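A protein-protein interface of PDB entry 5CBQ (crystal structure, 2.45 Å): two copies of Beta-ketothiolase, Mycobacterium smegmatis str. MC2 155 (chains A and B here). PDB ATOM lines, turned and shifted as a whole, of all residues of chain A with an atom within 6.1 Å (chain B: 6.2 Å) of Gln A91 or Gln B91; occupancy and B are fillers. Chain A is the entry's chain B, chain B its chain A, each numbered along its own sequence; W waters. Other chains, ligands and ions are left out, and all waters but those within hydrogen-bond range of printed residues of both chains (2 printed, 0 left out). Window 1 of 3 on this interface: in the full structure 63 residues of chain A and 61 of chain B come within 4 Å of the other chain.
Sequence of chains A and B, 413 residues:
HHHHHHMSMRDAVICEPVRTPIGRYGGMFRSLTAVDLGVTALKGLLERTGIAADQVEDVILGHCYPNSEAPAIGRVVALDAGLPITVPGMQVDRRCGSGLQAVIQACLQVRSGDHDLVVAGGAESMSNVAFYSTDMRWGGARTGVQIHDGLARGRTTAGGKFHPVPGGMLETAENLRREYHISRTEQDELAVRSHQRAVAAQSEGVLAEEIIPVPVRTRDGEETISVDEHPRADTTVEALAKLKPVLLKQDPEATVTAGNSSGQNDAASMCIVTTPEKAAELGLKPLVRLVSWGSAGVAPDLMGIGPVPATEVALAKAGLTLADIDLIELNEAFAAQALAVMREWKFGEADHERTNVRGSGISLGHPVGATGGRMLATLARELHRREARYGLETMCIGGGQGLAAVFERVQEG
Water W1 bridges O of Pro B66 and O of Pro A66.
Water W2 lies within hydrogen-bond range of OE1 of Gln A105 and SD of Met B90.
Among the printed residues, merely in contact across the chains: Pro A66 with Pro B66, Met A90 with Asp B93, Gln A91 with Val B92, Val A92 with Met B90, Val A92 with Gln B91, Val A92 with Val B92 and Asp A93 with Met B90.
Of the 18 printed residues of chain A, 8 touch a printed residue of chain B.
Of the 17 printed residues of chain B, 8 touch a printed residue of chain A.
Among the printed residues, 16 pairs touch across the chains.
Among the printed residues, no Asp or Glu carboxylate lies within 4 Å of a Lys or Arg side-chain nitrogen of the other chain.
Pro A66 touches its own counterpart, Pro B66.
Met A90 touches Arg B94, and with the chains exchanged Arg A94 touches Met B90.
Gln A91 touches Asp B93, and with the chains exchanged Asp A93 touches Gln B91.
Val A92 touches Met B90, but with the chains exchanged Met A90 does not touch Val B92 (4.1 Å).
Of the 16 pairs that touch across the chains among the printed residues, 15 have their exchanged pair printed and touching as well.
The side-chain carboxylate (OD1) of Asp B93 lies within hydrogen-bond range of the side-chain sulfur (SG) of Cys B64.
The backbone NH (N) of Leu A61 is in hydrogen-bond range of the backbone carbonyl oxygen (O) of Met A90, 3.3 Å away.
The backbone carbonyl oxygen of Val A92 lies within hydrogen-bond range of the backbone NH of His A63.
The backbone carbonyl oxygen of Val B59 is in hydrogen-bond range of the backbone NH of Met B90 (2.9 Å).
N of Val B92 is in hydrogen-bond range of O of Leu B61, 2.9 Å away.
The side-chain amide nitrogen (NE2) of Gln A91 lies within hydrogen-bond range of the backbone carbonyl oxygen (O) of His A63 (2.9 Å).
Printed residues of chain A within 4 Å of Gln B91: Gln A91 (3.1 Å), Val A92 (3.5 Å) and Asp A93 (3.0 Å).
Printed residues of chain B within 4 Å of Ala A72: Asp B93.
Of the printed residues of chain A, Met B90 touches Val A92, Asp A93 and Arg A94.
Ile A60 touches none of the printed residues of chain B.
Gly A74 touches none of the printed residues of chain B.
The nearest residue of chain A that does not touch Gln B91 is Pro A66 (5.0 Å).
The nearest printed residue of chain B that does not touch Met A90 is Val B92 (4.1 Å).
N of Gly A89 lies close to NH2 of Arg B94 (3.4 Å).
NH1 of Arg B94 lies within hydrogen-bond range of SD of Met A90 (3.4 Å).
The side-chain amide oxygen (OE1) of Gln B91 is in hydrogen-bond range of the side-chain amide nitrogen (NE2) of Gln A91 (3.1 Å).
The backbone NH (N) of Asp B93 sits at hydrogen-bond distance from the backbone carbonyl oxygen (O) of Gln A91, 3.0 Å away.
N of Ala B72 is in hydrogen-bond range of OD2 of Asp A93 (3.1 Å).
N of Ala A72 sits at hydrogen-bond distance from OD2 of Asp B93, at 3.2 Å.
The backbone NH (N) of Asp A93 is in hydrogen-bond range of the backbone carbonyl oxygen (O) of Gln B91, at 3.0 Å.
The guanidinium group of Arg A94 lies close to the backbone NH of Gly B89 (3.4 Å).
NH1 of Arg A94 sits at hydrogen-bond distance from SD of Met B90 (3.2 Å).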
ATOM      1  N   VAL A  59     -20.928   4.180  -0.271  1.00  0.00           N
ATOM      2  CA  VAL A  59     -21.212   5.413  -0.937  1.00  0.00           C
ATOM      3  C   VAL A  59     -21.075   6.489   0.108  1.00  0.00           C
ATOM      4  O   VAL A  59     -21.809   6.522   1.034  1.00  0.00           O
ATOM      5  CB  VAL A  59     -22.624   5.387  -1.552  1.00  0.00           C
ATOM      6  CG1 VAL A  59     -23.004   6.710  -2.117  1.00  0.00           C
ATOM      7  CG2 VAL A  59     -22.692   4.351  -2.611  1.00  0.00           C
ATOM      8  N   ILE A  60     -20.082   7.339  -0.050  1.00  0.00           N
ATOM      9  CA  ILE A  60     -19.788   8.391   0.910  1.00  0.00           C
ATOM     10  C   ILE A  60     -20.100   9.753   0.323  1.00  0.00           C
ATOM     11  O   ILE A  60     -19.574  10.125  -0.642  1.00  0.00           O
ATOM     12  CB  ILE A  60     -18.323   8.295   1.386  1.00  0.00           C
ATOM     13  CG1 ILE A  60     -18.021   6.873   1.884  1.00  0.00           C
ATOM     14  CG2 ILE A  60     -18.011   9.344   2.411  1.00  0.00           C
ATOM     15  CD1 ILE A  60     -16.583   6.512   1.776  1.00  0.00           C
ATOM     16  N   LEU A  61     -21.032  10.453   0.905  1.00  0.00           N
ATOM     17  CA  LEU A  61     -21.549  11.691   0.339  1.00  0.00           C
ATOM     18  C   LEU A  61     -21.466  12.908   1.212  1.00  0.00           C
ATOM     19  O   LEU A  61     -21.959  12.927   2.278  1.00  0.00           O
ATOM     20  CB  LEU A  61     -23.011  11.515  -0.070  1.00  0.00           C
ATOM     21  CG  LEU A  61     -23.360  11.162  -1.475  1.00  0.00           C
ATOM     22  CD1 LEU A  61     -22.336  10.307  -2.159  1.00  0.00           C
ATOM     23  CD2 LEU A  61     -24.709  10.504  -1.437  1.00  0.00           C
ATOM     24  N   GLY A  62     -20.906  13.958   0.673  1.00  0.00           N
ATOM     25  CA  GLY A  62     -20.840  15.213   1.341  1.00  0.00           C
ATOM     26  C   GLY A  62     -22.158  15.885   1.218  1.00  0.00           C
ATOM     27  O   GLY A  62     -22.654  16.050   0.168  1.00  0.00           O
ATOM     28  N   HIS A  63     -22.759  16.147   2.351  1.00  0.00           N
ATOM     29  CA  HIS A  63     -24.050  16.757   2.423  1.00  0.00           C
ATOM     30  C   HIS A  63     -24.112  17.790   3.548  1.00  0.00           C
ATOM     31  O   HIS A  63     -23.958  17.503   4.705  1.00  0.00           O
ATOM     32  CB  HIS A  63     -25.097  15.645   2.520  1.00  0.00           C
ATOM     33  CG  HIS A  63     -26.506  16.096   2.338  1.00  0.00           C
ATOM     34  ND1 HIS A  63     -26.897  16.925   1.328  1.00  0.00           N
ATOM     35  CD2 HIS A  63     -27.617  15.816   3.037  1.00  0.00           C
ATOM     36  CE1 HIS A  63     -28.180  17.171   1.440  1.00  0.00           C
ATOM     37  NE2 HIS A  63     -28.640  16.501   2.463  1.00  0.00           N
ATOM     38  N   CYS A  64     -24.315  19.026   3.170  1.00  0.00           N
ATOM     39  CA  CYS A  64     -24.295  20.113   4.126  1.00  0.00           C
ATOM     40  C   CYS A  64     -25.524  20.531   4.875  1.00  0.00           C
ATOM     41  O   CYS A  64     -25.406  21.105   5.891  1.00  0.00           O
ATOM     42  CB  CYS A  64     -23.660  21.312   3.495  1.00  0.00           C
ATOM     43  SG  CYS A  64     -21.977  20.997   3.132  1.00  0.00           S
ATOM     44  N   PRO A  66     -28.317  18.412   5.834  1.00  0.00           N
ATOM     45  CA  PRO A  66     -29.110  17.213   6.023  1.00  0.00           C
ATOM     46  C   PRO A  66     -30.367  17.404   6.877  1.00  0.00           C
ATOM     47  O   PRO A  66     -30.387  18.186   7.778  1.00  0.00           O
ATOM     48  CB  PRO A  66     -28.131  16.264   6.690  1.00  0.00           C
ATOM     49  CG  PRO A  66     -27.148  17.132   7.304  1.00  0.00           C
ATOM     50  CD  PRO A  66     -26.971  18.233   6.361  1.00  0.00           C
ATOM     51  N   PRO A  71     -31.820  10.595   5.937  1.00  0.00           N
ATOM     52  CA  PRO A  71     -30.749  10.248   6.861  1.00  0.00           C
ATOM     53  C   PRO A  71     -29.671   9.448   6.205  1.00  0.00           C
ATOM     54  O   PRO A  71     -30.002   8.683   5.336  1.00  0.00           O
ATOM     55  CB  PRO A  71     -31.453   9.342   7.843  1.00  0.00           C
ATOM     56  CG  PRO A  71     -32.804   9.794   7.844  1.00  0.00           C
ATOM     57  CD  PRO A  71     -33.104  10.128   6.444  1.00  0.00           C
ATOM     58  N   ALA A  72     -28.414   9.649   6.587  1.00  0.00           N
ATOM     59  CA  ALA A  72     -27.271   8.955   6.000  1.00  0.00           C
ATOM     60  C   ALA A  72     -27.277   8.928   4.492  1.00  0.00           C
ATOM     61  O   ALA A  72     -27.323   7.918   3.912  1.00  0.00           O
ATOM     62  CB  ALA A  72     -27.067   7.586   6.584  1.00  0.00           C
ATOM     63  N   ILE A  73     -27.216  10.064   3.873  1.00  0.00           N
ATOM     64  CA  ILE A  73     -27.790  10.255   2.587  1.00  0.00           C
ATOM     65  C   ILE A  73     -27.186   9.348   1.560  1.00  0.00           C
ATOM     66  O   ILE A  73     -27.791   9.035   0.599  1.00  0.00           O
ATOM     67  CB  ILE A  73     -27.774  11.728   2.162  1.00  0.00           C
ATOM     68  CG1 ILE A  73     -28.399  11.881   0.786  1.00  0.00           C
ATOM     69  CG2 ILE A  73     -26.371  12.299   2.246  1.00  0.00           C
ATOM     70  CD1 ILE A  73     -28.901  13.252   0.464  1.00  0.00           C
ATOM     71  N   GLY A  74     -25.989   8.906   1.820  1.00  0.00           N
ATOM     72  CA  GLY A  74     -25.317   8.012   0.929  1.00  0.00           C
ATOM     73  C   GLY A  74     -25.992   6.698   0.756  1.00  0.00           C
ATOM     74  O   GLY A  74     -26.033   6.183  -0.311  1.00  0.00           O
ATOM     75  N   GLY A  89     -23.741   3.141   2.906  1.00  0.00           N
ATOM     76  CA  GLY A  89     -23.544   4.532   2.603  1.00  0.00           C
ATOM     77  C   GLY A  89     -23.688   5.454   3.768  1.00  0.00           C
ATOM     78  O   GLY A  89     -24.239   5.092   4.713  1.00  0.00           O
ATOM     79  N   MET A  90     -23.226   6.679   3.635  1.00  0.00           N
ATOM     80  CA  MET A  90     -23.107   7.623   4.737  1.00  0.00           C
ATOM     81  C   MET A  90     -23.060   9.083   4.362  1.00  0.00           C
ATOM     82  O   MET A  90     -23.063   9.400   3.245  1.00  0.00           O
ATOM     83  CB  MET A  90     -21.933   7.266   5.625  1.00  0.00           C
ATOM     84  CG  MET A  90     -20.610   7.287   4.937  1.00  0.00           C
ATOM     85  SD  MET A  90     -19.218   7.343   6.033  1.00  0.00           S
ATOM     86  CE  MET A  90     -19.597   8.637   7.103  1.00  0.00           C
ATOM     87  N   GLN A  91     -23.013   9.959   5.340  1.00  0.00           N
ATOM     88  CA  GLN A  91     -22.941  11.378   5.096  1.00  0.00           C
ATOM     89  C   GLN A  91     -21.823  12.039   5.865  1.00  0.00           C
ATOM     90  O   GLN A  91     -21.528  11.667   6.947  1.00  0.00           O
ATOM     91  CB  GLN A  91     -24.294  12.029   5.357  1.00  0.00           C
ATOM     92  CG  GLN A  91     -24.348  13.525   5.291  1.00  0.00           C
ATOM     93  CD  GLN A  91     -24.215  14.156   6.641  1.00  0.00           C
ATOM     94  OE1 GLN A  91     -24.518  13.559   7.623  1.00  0.00           O
ATOM     95  NE2 GLN A  91     -23.768  15.344   6.685  1.00  0.00           N
ATOM     96  N   VAL A  92     -21.185  13.013   5.263  1.00  0.00           N
ATOM     97  CA  VAL A  92     -20.240  13.846   5.946  1.00  0.00           C
ATOM     98  C   VAL A  92     -20.447  15.326   5.671  1.00  0.00           C
ATOM     99  O   VAL A  92     -20.831  15.701   4.614  1.00  0.00           O
ATOM    100  CB  VAL A  92     -18.809  13.447   5.618  1.00  0.00           C
ATOM    101  CG1 VAL A  92     -18.537  12.054   6.079  1.00  0.00           C
ATOM    102  CG2 VAL A  92     -18.509  13.567   4.162  1.00  0.00           C
ATOM    103  N   ASP A  93     -20.191  16.148   6.666  1.00  0.00           N
ATOM    104  CA  ASP A  93     -20.129  17.594   6.553  1.00  0.00           C
ATOM    105  C   ASP A  93     -18.835  18.256   7.026  1.00  0.00           C
ATOM    106  O   ASP A  93     -18.493  18.172   8.145  1.00  0.00           O
ATOM    107  CB  ASP A  93     -21.320  18.221   7.276  1.00  0.00           C
ATOM    108  CG  ASP A  93     -21.348  19.719   7.212  1.00  0.00           C
ATOM    109  OD1 ASP A  93     -20.978  20.308   6.243  1.00  0.00           O
ATOM    110  OD2 ASP A  93     -21.780  20.341   8.142  1.00  0.00           O
ATOM    111  N   ARG A  94     -18.152  18.936   6.137  1.00  0.00           N
ATOM    112  CA  ARG A  94     -17.118  19.864   6.506  1.00  0.00           C
ATOM    113  C   ARG A  94     -17.315  21.138   5.722  1.00  0.00           C
ATOM    114  O   ARG A  94     -16.453  21.580   5.062  1.00  0.00           O
ATOM    115  CB  ARG A  94     -15.733  19.270   6.295  1.00  0.00           C
ATOM    116  CG  ARG A  94     -14.644  19.941   7.091  1.00  0.00           C
ATOM    117  CD  ARG A  94     -13.305  19.341   6.904  1.00  0.00           C
ATOM    118  NE  ARG A  94     -12.720  19.305   8.193  1.00  0.00           N
ATOM    119  CZ  ARG A  94     -12.257  18.244   8.783  1.00  0.00           C
ATOM    120  NH1 ARG A  94     -12.263  17.117   8.196  1.00  0.00           N
ATOM    121  NH2 ARG A  94     -11.808  18.341   9.988  1.00  0.00           N
ATOM    122  N   GLN A 105     -11.815  10.467   2.541  1.00  0.00           N
ATOM    123  CA  GLN A 105     -12.248   9.333   3.275  1.00  0.00           C
ATOM    124  C   GLN A 105     -12.225   8.105   2.414  1.00  0.00           C
ATOM    125  O   GLN A 105     -11.812   7.096   2.844  1.00  0.00           O
ATOM    126  CB  GLN A 105     -13.643   9.549   3.814  1.00  0.00           C
ATOM    127  CG  GLN A 105     -13.984   8.662   4.983  1.00  0.00           C
ATOM    128  CD  GLN A 105     -15.463   8.383   5.183  1.00  0.00           C
ATOM    129  OE1 GLN A 105     -16.192   9.216   5.599  1.00  0.00           O
ATOM    130  NE2 GLN A 105     -15.876   7.196   4.906  1.00  0.00           N
ATOM    131  N   VAL B  59     -11.335  17.242  15.087  1.00  0.00           N
ATOM    132  CA  VAL B  59     -12.370  16.761  15.929  1.00  0.00           C
ATOM    133  C   VAL B  59     -13.435  16.216  14.995  1.00  0.00           C
ATOM    134  O   VAL B  59     -14.034  16.946  14.280  1.00  0.00           O
ATOM    135  CB  VAL B  59     -12.906  17.865  16.850  1.00  0.00           C
ATOM    136  CG1 VAL B  59     -13.896  17.317  17.819  1.00  0.00           C
ATOM    137  CG2 VAL B  59     -11.807  18.505  17.617  1.00  0.00           C
ATOM    138  N   ILE B  60     -13.624  14.907  15.026  1.00  0.00           N
ATOM    139  CA  ILE B  60     -14.586  14.213  14.193  1.00  0.00           C
ATOM    140  C   ILE B  60     -15.738  13.720  15.041  1.00  0.00           C
ATOM    141  O   ILE B  60     -15.552  12.890  15.869  1.00  0.00           O
ATOM    142  CB  ILE B  60     -13.924  12.999  13.524  1.00  0.00           C
ATOM    143  CG1 ILE B  60     -12.645  13.405  12.824  1.00  0.00           C
ATOM    144  CG2 ILE B  60     -14.806  12.382  12.500  1.00  0.00           C
ATOM    145  CD1 ILE B  60     -11.721  12.270  12.512  1.00  0.00           C
ATOM    146  N   LEU B  61     -16.927  14.230  14.817  1.00  0.00           N
ATOM    147  CA  LEU B  61     -18.073  13.843  15.607  1.00  0.00           C
ATOM    148  C   LEU B  61     -19.221  13.166  14.870  1.00  0.00           C
ATOM    149  O   LEU B  61     -19.694  13.652  13.896  1.00  0.00           O
ATOM    150  CB  LEU B  61     -18.620  15.038  16.344  1.00  0.00           C
ATOM    151  CG  LEU B  61     -17.732  15.825  17.244  1.00  0.00           C
ATOM    152  CD1 LEU B  61     -18.556  16.842  17.968  1.00  0.00           C
ATOM    153  CD2 LEU B  61     -17.002  14.921  18.185  1.00  0.00           C
ATOM    154  N   GLY B  62     -19.677  12.053  15.425  1.00  0.00           N
ATOM    155  CA  GLY B  62     -20.884  11.381  15.034  1.00  0.00           C
ATOM    156  C   GLY B  62     -22.052  12.126  15.608  1.00  0.00           C
ATOM    157  O   GLY B  62     -22.106  12.306  16.740  1.00  0.00           O
ATOM    158  N   HIS B  63     -22.928  12.605  14.756  1.00  0.00           N
ATOM    159  CA  HIS B  63     -24.033  13.448  15.099  1.00  0.00           C
ATOM    160  C   HIS B  63     -25.174  13.216  14.108  1.00  0.00           C
ATOM    161  O   HIS B  63     -25.097  13.588  13.018  1.00  0.00           O
ATOM    162  CB  HIS B  63     -23.492  14.859  15.075  1.00  0.00           C
ATOM    163  CG  HIS B  63     -24.466  15.912  15.447  1.00  0.00           C
ATOM    164  ND1 HIS B  63     -25.131  15.931  16.634  1.00  0.00           N
ATOM    165  CD2 HIS B  63     -24.839  17.020  14.794  1.00  0.00           C
ATOM    166  CE1 HIS B  63     -25.892  16.996  16.687  1.00  0.00           C
ATOM    167  NE2 HIS B  63     -25.732  17.672  15.582  1.00  0.00           N
ATOM    168  N   CYS B  64     -26.247  12.578  14.513  1.00  0.00           N
ATOM    169  CA  CYS B  64     -27.344  12.203  13.624  1.00  0.00           C
ATOM    170  C   CYS B  64     -28.501  13.159  13.382  1.00  0.00           C
ATOM    171  O   CYS B  64     -29.263  12.926  12.520  1.00  0.00           O
ATOM    172  CB  CYS B  64     -27.901  10.883  14.068  1.00  0.00           C
ATOM    173  SG  CYS B  64     -26.708   9.581  14.153  1.00  0.00           S
ATOM    174  N   PRO B  66     -28.181  16.805  12.873  1.00  0.00           N
ATOM    175  CA  PRO B  66     -27.664  18.133  12.629  1.00  0.00           C
ATOM    176  C   PRO B  66     -28.639  19.148  12.091  1.00  0.00           C
ATOM    177  O   PRO B  66     -29.511  18.886  11.322  1.00  0.00           O
ATOM    178  CB  PRO B  66     -26.578  17.874  11.611  1.00  0.00           C
ATOM    179  CG  PRO B  66     -26.952  16.626  10.983  1.00  0.00           C
ATOM    180  CD  PRO B  66     -27.404  15.838  12.124  1.00  0.00           C
ATOM    181  N   PRO B  71     -23.331  23.971  12.534  1.00  0.00           N
ATOM    182  CA  PRO B  71     -22.825  23.281  11.338  1.00  0.00           C
ATOM    183  C   PRO B  71     -21.469  22.630  11.525  1.00  0.00           C
ATOM    184  O   PRO B  71     -20.690  23.181  12.217  1.00  0.00           O
ATOM    185  CB  PRO B  71     -22.681  24.404  10.325  1.00  0.00           C
ATOM    186  CG  PRO B  71     -23.372  25.530  10.886  1.00  0.00           C
ATOM    187  CD  PRO B  71     -23.271  25.410  12.349  1.00  0.00           C
ATOM    188  N   ALA B  72     -21.183  21.502  10.913  1.00  0.00           N
ATOM    189  CA  ALA B  72     -19.868  20.894  11.037  1.00  0.00           C
ATOM    190  C   ALA B  72     -19.363  20.731  12.471  1.00  0.00           C
ATOM    191  O   ALA B  72     -18.316  21.155  12.798  1.00  0.00           O
ATOM    192  CB  ALA B  72     -18.844  21.599  10.177  1.00  0.00           C
ATOM    193  N   ILE B  73     -20.117  20.034  13.276  1.00  0.00           N
ATOM    194  CA  ILE B  73     -20.236  20.191  14.692  1.00  0.00           C
ATOM    195  C   ILE B  73     -18.958  19.942  15.459  1.00  0.00           C
ATOM    196  O   ILE B  73     -18.809  20.431  16.500  1.00  0.00           O
ATOM    197  CB  ILE B  73     -21.443  19.400  15.232  1.00  0.00           C
ATOM    198  CG1 ILE B  73     -21.822  19.865  16.631  1.00  0.00           C
ATOM    199  CG2 ILE B  73     -21.212  17.922  15.144  1.00  0.00           C
ATOM    200  CD1 ILE B  73     -22.611  18.919  17.468  1.00  0.00           C
ATOM    201  N   GLY B  74     -18.032  19.208  14.897  1.00  0.00           N
ATOM    202  CA  GLY B  74     -16.732  19.045  15.475  1.00  0.00           C
ATOM    203  C   GLY B  74     -15.956  20.329  15.567  1.00  0.00           C
ATOM    204  O   GLY B  74     -15.331  20.576  16.537  1.00  0.00           O
ATOM    205  N   GLY B  89     -12.567  20.672  12.393  1.00  0.00           N
ATOM    206  CA  GLY B  89     -13.586  19.775  12.859  1.00  0.00           C
ATOM    207  C   GLY B  89     -14.667  19.459  11.885  1.00  0.00           C
ATOM    208  O   GLY B  89     -14.893  20.167  10.991  1.00  0.00           O
ATOM    209  N   MET B  90     -15.349  18.357  12.094  1.00  0.00           N
ATOM    210  CA  MET B  90     -16.342  17.848  11.143  1.00  0.00           C
ATOM    211  C   MET B  90     -17.484  16.993  11.721  1.00  0.00           C
ATOM    212  O   MET B  90     -17.464  16.632  12.832  1.00  0.00           O
ATOM    213  CB  MET B  90     -15.676  17.199   9.918  1.00  0.00           C
ATOM    214  CG  MET B  90     -14.950  15.889  10.119  1.00  0.00           C
ATOM    215  SD  MET B  90     -14.642  15.015   8.605  1.00  0.00           S
ATOM    216  CE  MET B  90     -16.222  14.788   7.947  1.00  0.00           C
ATOM    217  N   GLN B  91     -18.483  16.687  10.916  1.00  0.00           N
ATOM    218  CA  GLN B  91     -19.608  15.869  11.314  1.00  0.00           C
ATOM    219  C   GLN B  91     -19.817  14.676  10.413  1.00  0.00           C
ATOM    220  O   GLN B  91     -19.760  14.783   9.260  1.00  0.00           O
ATOM    221  CB  GLN B  91     -20.881  16.700  11.453  1.00  0.00           C
ATOM    222  CG  GLN B  91     -22.148  15.933  11.756  1.00  0.00           C
ATOM    223  CD  GLN B  91     -22.877  15.553  10.511  1.00  0.00           C
ATOM    224  OE1 GLN B  91     -22.798  16.230   9.543  1.00  0.00           O
ATOM    225  NE2 GLN B  91     -23.519  14.474  10.528  1.00  0.00           N
ATOM    226  N   VAL B  92     -20.069  13.526  10.983  1.00  0.00           N
ATOM    227  CA  VAL B  92     -20.413  12.351  10.230  1.00  0.00           C
ATOM    228  C   VAL B  92     -21.679  11.651  10.674  1.00  0.00           C
ATOM    229  O   VAL B  92     -21.989  11.630  11.820  1.00  0.00           O
ATOM    230  CB  VAL B  92     -19.277  11.339  10.169  1.00  0.00           C
ATOM    231  CG1 VAL B  92     -18.118  11.912   9.431  1.00  0.00           C
ATOM    232  CG2 VAL B  92     -18.904  10.812  11.517  1.00  0.00           C
ATOM    233  N   ASP B  93     -22.410  11.116   9.709  1.00  0.00           N
ATOM    234  CA  ASP B  93     -23.614  10.351   9.946  1.00  0.00           C
ATOM    235  C   ASP B  93     -23.687   9.004   9.230  1.00  0.00           C
ATOM    236  O   ASP B  93     -23.783   8.905   8.058  1.00  0.00           O
ATOM    237  CB  ASP B  93     -24.823  11.242   9.648  1.00  0.00           C
ATOM    238  CG  ASP B  93     -26.176  10.559   9.801  1.00  0.00           C
ATOM    239  OD1 ASP B  93     -26.353   9.655  10.571  1.00  0.00           O
ATOM    240  OD2 ASP B  93     -27.112  10.975   9.151  1.00  0.00           O
ATOM    241  N   ARG B  94     -23.648   7.974  10.032  1.00  0.00           N
ATOM    242  CA  ARG B  94     -24.029   6.647   9.684  1.00  0.00           C
ATOM    243  C   ARG B  94     -25.018   6.101  10.706  1.00  0.00           C
ATOM    244  O   ARG B  94     -24.874   5.016  11.177  1.00  0.00           O
ATOM    245  CB  ARG B  94     -22.836   5.756   9.569  1.00  0.00           C
ATOM    246  CG  ARG B  94     -23.068   4.634   8.607  1.00  0.00           C
ATOM    247  CD  ARG B  94     -21.825   3.895   8.292  1.00  0.00           C
ATOM    248  NE  ARG B  94     -21.833   3.675   6.886  1.00  0.00           N
ATOM    249  CZ  ARG B  94     -20.799   3.749   6.095  1.00  0.00           C
ATOM    250  NH1 ARG B  94     -19.632   4.035   6.558  1.00  0.00           N
ATOM    251  NH2 ARG B  94     -20.957   3.526   4.829  1.00  0.00           N
HETATM  252  O   HOH W   1     -30.677  16.484  10.714  1.00  0.00           O
HETATM  253  O   HOH W   2     -14.817  11.923   6.499  1.00  0.00           O
